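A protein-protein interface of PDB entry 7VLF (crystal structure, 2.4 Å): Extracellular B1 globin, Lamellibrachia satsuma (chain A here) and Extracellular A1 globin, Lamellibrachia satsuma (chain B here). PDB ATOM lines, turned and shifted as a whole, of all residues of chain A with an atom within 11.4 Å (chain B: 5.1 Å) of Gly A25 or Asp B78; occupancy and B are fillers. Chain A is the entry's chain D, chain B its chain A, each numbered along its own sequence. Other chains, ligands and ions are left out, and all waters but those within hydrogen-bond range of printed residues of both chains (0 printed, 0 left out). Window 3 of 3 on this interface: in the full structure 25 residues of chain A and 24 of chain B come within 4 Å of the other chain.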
ATOM      1  N   ASN A  17       0.541 -12.547  16.464  1.00  0.00           N
ATOM      2  CA  ASN A  17      -0.281 -13.133  15.410  1.00  0.00           C
ATOM      3  C   ASN A  17      -0.232 -12.305  14.133  1.00  0.00           C
ATOM      4  O   ASN A  17      -0.468 -12.836  13.043  1.00  0.00           O
ATOM      5  CB  ASN A  17      -1.726 -13.276  15.896  1.00  0.00           C
ATOM      6  CG  ASN A  17      -2.632 -13.940  14.870  1.00  0.00           C
ATOM      7  OD1 ASN A  17      -2.761 -15.164  14.838  1.00  0.00           O
ATOM      8  ND2 ASN A  17      -3.265 -13.130  14.028  1.00  0.00           N
ATOM      9  N   GLN A  18       0.076 -11.011  14.249  1.00  0.00           N
ATOM     10  CA  GLN A  18       0.160 -10.154  13.070  1.00  0.00           C
ATOM     11  C   GLN A  18       1.250 -10.626  12.117  1.00  0.00           C
ATOM     12  O   GLN A  18       1.082 -10.577  10.894  1.00  0.00           O
ATOM     13  CB  GLN A  18       0.413  -8.707  13.497  1.00  0.00           C
ATOM     14  CG  GLN A  18       0.655  -7.747  12.346  1.00  0.00           C
ATOM     15  CD  GLN A  18       1.100  -6.379  12.821  1.00  0.00           C
ATOM     16  OE1 GLN A  18       1.163  -5.426  12.044  1.00  0.00           O
ATOM     17  NE2 GLN A  18       1.412  -6.275  14.106  1.00  0.00           N
ATOM     18  N   ILE A  19       2.373 -11.093  12.659  1.00  0.00           N
ATOM     19  CA  ILE A  19       3.510 -11.511  11.845  1.00  0.00           C
ATOM     20  C   ILE A  19       3.680 -13.019  11.783  1.00  0.00           C
ATOM     21  O   ILE A  19       4.551 -13.492  11.037  1.00  0.00           O
ATOM     22  CB  ILE A  19       4.820 -10.861  12.335  1.00  0.00           C
ATOM     23  CG1 ILE A  19       5.070 -11.229  13.799  1.00  0.00           C
ATOM     24  CG2 ILE A  19       4.770  -9.358  12.152  1.00  0.00           C
ATOM     25  CD1 ILE A  19       6.510 -11.591  14.100  1.00  0.00           C
ATOM     26  N   TYR A  20       2.901 -13.789  12.541  1.00  0.00           N
ATOM     27  CA  TYR A  20       3.051 -15.241  12.572  1.00  0.00           C
ATOM     28  C   TYR A  20       1.681 -15.888  12.705  1.00  0.00           C
ATOM     29  O   TYR A  20       1.084 -15.870  13.786  1.00  0.00           O
ATOM     30  CB  TYR A  20       3.973 -15.677  13.715  1.00  0.00           C
ATOM     31  CG  TYR A  20       4.379 -17.136  13.661  1.00  0.00           C
ATOM     32  CD1 TYR A  20       3.507 -18.139  14.071  1.00  0.00           C
ATOM     33  CD2 TYR A  20       5.639 -17.511  13.214  1.00  0.00           C
ATOM     34  CE1 TYR A  20       3.874 -19.474  14.021  1.00  0.00           C
ATOM     35  CE2 TYR A  20       6.016 -18.842  13.166  1.00  0.00           C
ATOM     36  CZ  TYR A  20       5.129 -19.819  13.573  1.00  0.00           C
ATOM     37  OH  TYR A  20       5.499 -21.146  13.527  1.00  0.00           O
ATOM     38  N   ASN A  21       1.186 -16.455  11.609  1.00  0.00           N
ATOM     39  CA  ASN A  21       0.029 -17.332  11.634  1.00  0.00           C
ATOM     40  C   ASN A  21       0.282 -18.470  10.654  1.00  0.00           C
ATOM     41  O   ASN A  21       1.360 -18.578  10.060  1.00  0.00           O
ATOM     42  CB  ASN A  21      -1.266 -16.585  11.293  1.00  0.00           C
ATOM     43  CG  ASN A  21      -1.271 -16.038   9.877  1.00  0.00           C
ATOM     44  OD1 ASN A  21      -1.624 -16.739   8.927  1.00  0.00           O
ATOM     45  ND2 ASN A  21      -0.877 -14.780   9.730  1.00  0.00           N
ATOM     46  N   ALA A  22      -0.727 -19.324  10.475  1.00  0.00           N
ATOM     47  CA  ALA A  22      -0.548 -20.494   9.626  1.00  0.00           C
ATOM     48  C   ALA A  22      -0.597 -20.148   8.143  1.00  0.00           C
ATOM     49  O   ALA A  22       0.119 -20.764   7.346  1.00  0.00           O
ATOM     50  CB  ALA A  22      -1.603 -21.549   9.958  1.00  0.00           C
ATOM     51  N   GLY A  23      -1.410 -19.167   7.756  1.00  0.00           N
ATOM     52  CA  GLY A  23      -1.582 -18.837   6.354  1.00  0.00           C
ATOM     53  C   GLY A  23      -0.413 -18.137   5.699  1.00  0.00           C
ATOM     54  O   GLY A  23      -0.531 -17.719   4.543  1.00  0.00           O
ATOM     55  N   ILE A  24       0.713 -18.004   6.391  1.00  0.00           N
ATOM     56  CA  ILE A  24       1.861 -17.295   5.839  1.00  0.00           C
ATOM     57  C   ILE A  24       2.653 -18.225   4.933  1.00  0.00           C
ATOM     58  O   ILE A  24       2.840 -19.411   5.234  1.00  0.00           O
ATOM     59  CB  ILE A  24       2.738 -16.729   6.968  1.00  0.00           C
ATOM     60  CG1 ILE A  24       1.878 -15.945   7.960  1.00  0.00           C
ATOM     61  CG2 ILE A  24       3.834 -15.835   6.400  1.00  0.00           C
ATOM     62  CD1 ILE A  24       2.681 -15.147   8.959  1.00  0.00           C
ATOM     63  N   GLY A  25       3.124 -17.685   3.810  1.00  0.00           N
ATOM     64  CA  GLY A  25       3.958 -18.469   2.922  1.00  0.00           C
ATOM     65  C   GLY A  25       5.246 -18.898   3.600  1.00  0.00           C
ATOM     66  O   GLY A  25       5.793 -18.192   4.450  1.00  0.00           O
ATOM     67  N   ALA A  26       5.730 -20.080   3.213  1.00  0.00           N
ATOM     68  CA  ALA A  26       6.907 -20.650   3.860  1.00  0.00           C
ATOM     69  C   ALA A  26       8.143 -19.786   3.652  1.00  0.00           C
ATOM     70  O   ALA A  26       9.066 -19.820   4.473  1.00  0.00           O
ATOM     71  CB  ALA A  26       7.160 -22.064   3.340  1.00  0.00           C
ATOM     72  N   LYS A  27       8.181 -19.008   2.569  1.00  0.00           N
ATOM     73  CA  LYS A  27       9.346 -18.172   2.304  1.00  0.00           C
ATOM     74  C   LYS A  27       9.510 -17.097   3.371  1.00  0.00           C
ATOM     75  O   LYS A  27      10.635 -16.773   3.770  1.00  0.00           O
ATOM     76  CB  LYS A  27       9.231 -17.547   0.914  1.00  0.00           C
ATOM     77  CG  LYS A  27      10.428 -16.714   0.491  1.00  0.00           C
ATOM     78  CD  LYS A  27      10.739 -16.932  -0.981  1.00  0.00           C
ATOM     79  CE  LYS A  27       9.481 -16.854  -1.831  1.00  0.00           C
ATOM     80  NZ  LYS A  27       9.743 -17.256  -3.240  1.00  0.00           N
ATOM     81  N   SER A  28       8.397 -16.533   3.846  1.00  0.00           N
ATOM     82  CA  SER A  28       8.475 -15.554   4.923  1.00  0.00           C
ATOM     83  C   SER A  28       8.874 -16.209   6.237  1.00  0.00           C
ATOM     84  O   SER A  28       9.513 -15.569   7.079  1.00  0.00           O
ATOM     85  CB  SER A  28       7.141 -14.822   5.065  1.00  0.00           C
ATOM     86  OG  SER A  28       7.254 -13.730   5.959  1.00  0.00           O
ATOM     87  N   ARG A  29       8.530 -17.486   6.420  1.00  0.00           N
ATOM     88  CA  ARG A  29       8.953 -18.194   7.622  1.00  0.00           C
ATOM     89  C   ARG A  29      10.449 -18.503   7.596  1.00  0.00           C
ATOM     90  O   ARG A  29      11.064 -18.644   8.658  1.00  0.00           O
ATOM     91  CB  ARG A  29       8.137 -19.479   7.787  1.00  0.00           C
ATOM     92  CG  ARG A  29       6.702 -19.376   7.302  1.00  0.00           C
ATOM     93  CD  ARG A  29       5.926 -20.633   7.641  1.00  0.00           C
ATOM     94  NE  ARG A  29       5.455 -20.622   9.021  1.00  0.00           N
ATOM     95  CZ  ARG A  29       4.257 -20.181   9.390  1.00  0.00           C
ATOM     96  NH1 ARG A  29       3.415 -19.721   8.476  1.00  0.00           N
ATOM     97  NH2 ARG A  29       3.896 -20.203  10.665  1.00  0.00           N
ATOM     98  N   TRP A  30      11.056 -18.605   6.404  1.00  0.00           N
ATOM     99  CA  TRP A  30      12.497 -18.862   6.311  1.00  0.00           C
ATOM    100  C   TRP A  30      13.314 -17.596   6.525  1.00  0.00           C
ATOM    101  O   TRP A  30      14.356 -17.631   7.189  1.00  0.00           O
ATOM    102  CB  TRP A  30      12.853 -19.498   4.959  1.00  0.00           C
ATOM    103  CG  TRP A  30      12.123 -20.784   4.674  1.00  0.00           C
ATOM    104  CD1 TRP A  30      11.696 -21.247   3.457  1.00  0.00           C
ATOM    105  CD2 TRP A  30      11.728 -21.770   5.636  1.00  0.00           C
ATOM    106  NE1 TRP A  30      11.063 -22.461   3.609  1.00  0.00           N
ATOM    107  CE2 TRP A  30      11.072 -22.800   4.938  1.00  0.00           C
ATOM    108  CE3 TRP A  30      11.872 -21.883   7.024  1.00  0.00           C
ATOM    109  CZ2 TRP A  30      10.555 -23.920   5.587  1.00  0.00           C
ATOM    110  CZ3 TRP A  30      11.364 -22.980   7.655  1.00  0.00           C
ATOM    111  CH2 TRP A  30      10.713 -23.990   6.947  1.00  0.00           C
ATOM    112  N   THR A  31      12.854 -16.478   5.973  1.00  0.00           N
ATOM    113  CA  THR A  31      13.494 -15.198   6.247  1.00  0.00           C
ATOM    114  C   THR A  31      13.601 -14.952   7.748  1.00  0.00           C
ATOM    115  O   THR A  31      14.600 -14.402   8.227  1.00  0.00           O
ATOM    116  CB  THR A  31      12.706 -14.071   5.567  1.00  0.00           C
ATOM    117  OG1 THR A  31      12.668 -14.296   4.152  1.00  0.00           O
ATOM    118  CG2 THR A  31      13.328 -12.712   5.835  1.00  0.00           C
ATOM    119  N   MET A  32      12.573 -15.343   8.505  1.00  0.00           N
ATOM    120  CA  MET A  32      12.610 -15.173   9.954  1.00  0.00           C
ATOM    121  C   MET A  32      13.613 -16.121  10.604  1.00  0.00           C
ATOM    122  O   MET A  32      14.343 -15.729  11.522  1.00  0.00           O
ATOM    123  CB  MET A  32      11.213 -15.385  10.537  1.00  0.00           C
ATOM    124  CG  MET A  32      10.170 -14.400  10.029  1.00  0.00           C
ATOM    125  SD  MET A  32       8.511 -14.789  10.623  1.00  0.00           S
ATOM    126  CE  MET A  32       8.754 -14.690  12.397  1.00  0.00           C
ATOM    127  N   GLY A  33      13.665 -17.373  10.146  1.00  0.00           N
ATOM    128  CA  GLY A  33      14.544 -18.344  10.780  1.00  0.00           C
ATOM    129  C   GLY A  33      16.011 -17.983  10.649  1.00  0.00           C
ATOM    130  O   GLY A  33      16.760 -18.004  11.629  1.00  0.00           O
ATOM    131  N   GLY A  62      16.467 -27.796   3.959  1.00  0.00           N
ATOM    132  CA  GLY A  62      15.149 -28.074   4.499  1.00  0.00           C
ATOM    133  C   GLY A  62      15.193 -28.634   5.905  1.00  0.00           C
ATOM    134  O   GLY A  62      14.232 -28.492   6.666  1.00  0.00           O
ATOM    135  N   HIS A  65      15.733 -25.491   8.001  1.00  0.00           N
ATOM    136  CA  HIS A  65      14.447 -24.815   7.876  1.00  0.00           C
ATOM    137  C   HIS A  65      13.409 -25.438   8.800  1.00  0.00           C
ATOM    138  O   HIS A  65      12.785 -24.739   9.606  1.00  0.00           O
ATOM    139  CB  HIS A  65      13.978 -24.850   6.420  1.00  0.00           C
ATOM    140  CG  HIS A  65      14.524 -23.743   5.572  1.00  0.00           C
ATOM    141  ND1 HIS A  65      14.235 -23.628   4.227  1.00  0.00           N
ATOM    142  CD2 HIS A  65      15.335 -22.701   5.876  1.00  0.00           C
ATOM    143  CE1 HIS A  65      14.848 -22.564   3.742  1.00  0.00           C
ATOM    144  NE2 HIS A  65      15.522 -21.985   4.720  1.00  0.00           N
ATOM    145  N   ALA A  66      13.241 -26.761   8.731  1.00  0.00           N
ATOM    146  CA  ALA A  66      12.249 -27.415   9.576  1.00  0.00           C
ATOM    147  C   ALA A  66      12.573 -27.257  11.055  1.00  0.00           C
ATOM    148  O   ALA A  66      11.666 -27.296  11.894  1.00  0.00           O
ATOM    149  CB  ALA A  66      12.131 -28.899   9.221  1.00  0.00           C
ATOM    150  N   THR A  68      13.997 -24.455  12.472  1.00  0.00           N
ATOM    151  CA  THR A  68      13.597 -23.113  12.878  1.00  0.00           C
ATOM    152  C   THR A  68      12.089 -23.009  13.063  1.00  0.00           C
ATOM    153  O   THR A  68      11.620 -22.235  13.905  1.00  0.00           O
ATOM    154  CB  THR A  68      14.077 -22.085  11.854  1.00  0.00           C
ATOM    155  OG1 THR A  68      13.527 -22.395  10.568  1.00  0.00           O
ATOM    156  CG2 THR A  68      15.595 -22.100  11.766  1.00  0.00           C
ATOM    157  N   VAL A  69      11.316 -23.779  12.296  1.00  0.00           N
ATOM    158  CA  VAL A  69       9.868 -23.766  12.463  1.00  0.00           C
ATOM    159  C   VAL A  69       9.476 -24.435  13.772  1.00  0.00           C
ATOM    160  O   VAL A  69       8.586 -23.958  14.486  1.00  0.00           O
ATOM    161  CB  VAL A  69       9.186 -24.431  11.255  1.00  0.00           C
ATOM    162  CG1 VAL A  69       7.774 -24.835  11.607  1.00  0.00           C
ATOM    163  CG2 VAL A  69       9.165 -23.476  10.092  1.00  0.00           C
ATOM    164  N   LEU A  72       9.974 -21.877  16.316  1.00  0.00           N
ATOM    165  CA  LEU A  72       8.968 -20.823  16.227  1.00  0.00           C
ATOM    166  C   LEU A  72       7.581 -21.347  16.574  1.00  0.00           C
ATOM    167  O   LEU A  72       6.776 -20.628  17.177  1.00  0.00           O
ATOM    168  CB  LEU A  72       8.974 -20.200  14.832  1.00  0.00           C
ATOM    169  CG  LEU A  72      10.212 -19.369  14.494  1.00  0.00           C
ATOM    170  CD1 LEU A  72      10.097 -18.724  13.118  1.00  0.00           C
ATOM    171  CD2 LEU A  72      10.444 -18.318  15.566  1.00  0.00           C
ATOM    172  N   ILE B   4      -0.716 -27.981  -5.146  1.00  0.00           N
ATOM    173  CA  ILE B   4      -0.352 -26.735  -4.476  1.00  0.00           C
ATOM    174  C   ILE B   4      -1.593 -25.910  -4.153  1.00  0.00           C
ATOM    175  O   ILE B   4      -1.652 -25.238  -3.115  1.00  0.00           O
ATOM    176  CB  ILE B   4       0.659 -25.945  -5.330  1.00  0.00           C
ATOM    177  CG1 ILE B   4       1.047 -24.638  -4.633  1.00  0.00           C
ATOM    178  CG2 ILE B   4       0.107 -25.682  -6.723  1.00  0.00           C
ATOM    179  CD1 ILE B   4       1.683 -24.841  -3.271  1.00  0.00           C
ATOM    180  N   ARG B   7      -3.059 -27.344  -1.098  1.00  0.00           N
ATOM    181  CA  ARG B   7      -2.194 -26.984   0.021  1.00  0.00           C
ATOM    182  C   ARG B   7      -2.455 -25.556   0.485  1.00  0.00           C
ATOM    183  O   ARG B   7      -2.534 -25.293   1.690  1.00  0.00           O
ATOM    184  CB  ARG B   7      -0.727 -27.163  -0.371  1.00  0.00           C
ATOM    185  CG  ARG B   7      -0.289 -28.612  -0.477  1.00  0.00           C
ATOM    186  CD  ARG B   7       0.968 -28.758  -1.321  1.00  0.00           C
ATOM    187  NE  ARG B   7       1.295 -30.161  -1.560  1.00  0.00           N
ATOM    188  CZ  ARG B   7       2.108 -30.879  -0.792  1.00  0.00           C
ATOM    189  NH1 ARG B   7       2.685 -30.325   0.265  1.00  0.00           N
ATOM    190  NH2 ARG B   7       2.347 -32.151  -1.081  1.00  0.00           N
ATOM    191  N   LEU B   8      -2.599 -24.620  -0.455  1.00  0.00           N
ATOM    192  CA  LEU B   8      -2.873 -23.241  -0.068  1.00  0.00           C
ATOM    193  C   LEU B   8      -4.284 -23.092   0.485  1.00  0.00           C
ATOM    194  O   LEU B   8      -4.510 -22.316   1.420  1.00  0.00           O
ATOM    195  CB  LEU B   8      -2.659 -22.304  -1.256  1.00  0.00           C
ATOM    196  CG  LEU B   8      -1.215 -22.160  -1.735  1.00  0.00           C
ATOM    197  CD1 LEU B   8      -1.117 -21.098  -2.815  1.00  0.00           C
ATOM    198  CD2 LEU B   8      -0.291 -21.834  -0.571  1.00  0.00           C
ATOM    199  N   LYS B  11      -4.326 -24.333   4.084  1.00  0.00           N
ATOM    200  CA  LYS B  11      -3.741 -23.369   5.010  1.00  0.00           C
ATOM    201  C   LYS B  11      -4.730 -22.265   5.361  1.00  0.00           C
ATOM    202  O   LYS B  11      -4.831 -21.860   6.525  1.00  0.00           O
ATOM    203  CB  LYS B  11      -2.465 -22.774   4.416  1.00  0.00           C
ATOM    204  CG  LYS B  11      -1.361 -23.791   4.178  1.00  0.00           C
ATOM    205  CD  LYS B  11      -0.141 -23.151   3.536  1.00  0.00           C
ATOM    206  CE  LYS B  11       0.573 -22.229   4.508  1.00  0.00           C
ATOM    207  NZ  LYS B  11       1.740 -21.548   3.885  1.00  0.00           N
ATOM    208  N   SER B  75       1.762 -25.219   7.846  1.00  0.00           N
ATOM    209  CA  SER B  75       2.411 -23.995   7.392  1.00  0.00           C
ATOM    210  C   SER B  75       3.482 -24.278   6.349  1.00  0.00           C
ATOM    211  O   SER B  75       3.747 -23.431   5.489  1.00  0.00           O
ATOM    212  CB  SER B  75       3.016 -23.256   8.585  1.00  0.00           C
ATOM    213  OG  SER B  75       2.023 -22.949   9.547  1.00  0.00           O
ATOM    214  N   MET B  76       4.106 -25.455   6.407  1.00  0.00           N
ATOM    215  CA  MET B  76       5.124 -25.849   5.445  1.00  0.00           C
ATOM    216  C   MET B  76       4.561 -26.710   4.316  1.00  0.00           C
ATOM    217  O   MET B  76       5.318 -27.447   3.675  1.00  0.00           O
ATOM    218  CB  MET B  76       6.262 -26.586   6.152  1.00  0.00           C
ATOM    219  CG  MET B  76       7.020 -25.743   7.164  1.00  0.00           C
ATOM    220  SD  MET B  76       8.305 -26.691   8.004  1.00  0.00           S
ATOM    221  CE  MET B  76       7.312 -27.974   8.758  1.00  0.00           C
ATOM    222  N   PHE B  77       3.250 -26.631   4.062  1.00  0.00           N
ATOM    223  CA  PHE B  77       2.643 -27.429   2.998  1.00  0.00           C
ATOM    224  C   PHE B  77       3.213 -27.069   1.634  1.00  0.00           C
ATOM    225  O   PHE B  77       3.401 -27.943   0.779  1.00  0.00           O
ATOM    226  CB  PHE B  77       1.126 -27.241   3.004  1.00  0.00           C
ATOM    227  CG  PHE B  77       0.371 -28.409   3.565  1.00  0.00           C
ATOM    228  CD1 PHE B  77       0.684 -29.707   3.182  1.00  0.00           C
ATOM    229  CD2 PHE B  77      -0.663 -28.208   4.462  1.00  0.00           C
ATOM    230  CE1 PHE B  77      -0.022 -30.786   3.700  1.00  0.00           C
ATOM    231  CE2 PHE B  77      -1.368 -29.272   4.986  1.00  0.00           C
ATOM    232  CZ  PHE B  77      -1.050 -30.564   4.606  1.00  0.00           C
ATOM    233  N   ASP B  78       3.511 -25.788   1.417  1.00  0.00           N
ATOM    234  CA  ASP B  78       3.977 -25.350   0.108  1.00  0.00           C
ATOM    235  C   ASP B  78       5.383 -25.857  -0.187  1.00  0.00           C
ATOM    236  O   ASP B  78       5.672 -26.274  -1.315  1.00  0.00           O
ATOM    237  CB  ASP B  78       3.925 -23.827   0.022  1.00  0.00           C
ATOM    238  CG  ASP B  78       4.351 -23.159   1.310  1.00  0.00           C
ATOM    239  OD1 ASP B  78       4.652 -23.888   2.278  1.00  0.00           O
ATOM    240  OD2 ASP B  78       4.381 -21.912   1.358  1.00  0.00           O
ATOM    241  N   ASN B  79       6.271 -25.827   0.802  1.00  0.00           N
ATOM    242  CA  ASN B  79       7.662 -26.201   0.589  1.00  0.00           C
ATOM    243  C   ASN B  79       7.857 -27.664   0.976  1.00  0.00           C
ATOM    244  O   ASN B  79       7.534 -28.064   2.101  1.00  0.00           O
ATOM    245  CB  ASN B  79       8.582 -25.287   1.396  1.00  0.00           C
ATOM    246  CG  ASN B  79      10.033 -25.694   1.308  1.00  0.00           C
ATOM    247  OD1 ASN B  79      10.762 -25.268   0.410  1.00  0.00           O
ATOM    248  ND2 ASN B  79      10.466 -26.516   2.247  1.00  0.00           N
ATOM    249  N   GLU B  80       8.381 -28.461   0.042  1.00  0.00           N
ATOM    250  CA  GLU B  80       8.499 -29.899   0.269  1.00  0.00           C
ATOM    251  C   GLU B  80       9.705 -30.244   1.133  1.00  0.00           C
ATOM    252  O   GLU B  80       9.634 -31.167   1.952  1.00  0.00           O
ATOM    253  CB  GLU B  80       8.585 -30.638  -1.067  1.00  0.00           C
ATOM    254  CG  GLU B  80       7.251 -30.807  -1.777  1.00  0.00           C
ATOM    255  CD  GLU B  80       6.405 -31.914  -1.184  1.00  0.00           C
ATOM    256  OE1 GLU B  80       6.964 -32.990  -0.878  1.00  0.00           O
ATOM    257  OE2 GLU B  80       5.181 -31.709  -1.026  1.00  0.00           O
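Hydrophobic or aromatic side chains of chain B within 4 Å of the printed part of chain A: Met B76.
Hydrophobic or aromatic side chains of chain A within 4 Å of the printed part of chain B: Ala A22, Ala A26, Trp A30 and Val A69.
Among the printed residues, no Asp or Glu carboxylate lies within 4 Å of a Lys or Arg side-chain nitrogen of the other chain.
Gly A25 touches just these residues of chain B: Lys B11 (3.9 Å) and Asp B78 (3.8 Å).
Printed residues of chain A within 4 Å of Asp B78: Gly A25 (3.8 Å) and Ala A26 (2.9 Å).
No residue of chain A comes within 4 Å of Arg B7.
No residue of chain A comes within 4 Å of Phe B77.
No residue of chain A comes within 4 Å of Asn B79.
No residue of chain A comes within 4 Å of Glu B80.
Of the printed residues of chain A, Met B76 touches Trp A30 (3.8 Å) and Val A69 (3.9 Å).
Of the printed residues of chain B, Ala A26 touches Asp B78 (2.9 Å).
Printed residues of chain B within 4 Å of Trp A30: Met B76.
Printed residues of chain B within 4 Å of Ala A22: Lys B11 (3.2 Å) and Ser B75 (3.6 Å).
Of the printed residues of chain B, Ile A24 touches Lys B11.
Ser A28 touches none of the printed residues of chain B.
The nearest printed residue of chain B that does not touch Gly A25 is Ser B75 (5.1 Å).
The nearest residue of chain A that does not touch Asp B78 is Ile A24 (4.9 Å).
Lys B11 touches Ala A22 (CE to O, 3.2 Å).
Ser B75 touches Ala A22 (OG to CA, 3.6 Å).
Gly A25 touches Lys B11 (CA to NZ, 3.9 Å).
Gly A25 touches Asp B78 (CA to OD2, 3.8 Å).
CZ of Arg A29 touches CB of Ser B75, at 3.4 Å.
Trp A30 touches Met B76.
SD of Met B76 touches CG2 of Val A69 (3.9 Å).
The side-chain amino group (NZ) of Lys B11 is in hydrogen-bond range of the backbone carbonyl oxygen (O) of Ile A24.
The side-chain carboxylate (OD2) of Asp B78 lies within hydrogen-bond range of the backbone NH (N) of Ala A26 (2.9 Å).
NH1 of Arg A29 lies within hydrogen-bond range of O of Ile A24 (3.3 Å).
The side-chain amino group (NZ) of Lys B11 is in hydrogen-bond range of the backbone carbonyl oxygen (O) of Ser B75 (3.2 Å).
OH of Tyr A20 sits close to NH2 of Arg A29.
O of Ala A26 sits close to NE1 of Trp A30.
The indole nitrogen (NE1) of Trp A30 sits close to a ring nitrogen (ND1) of His A65 (3.4 Å).
The side-chain amino group (NZ) of Lys B11 lies within salt-bridge range of the side-chain carboxylate (OD2) of Asp B78, 3.7 Å away.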
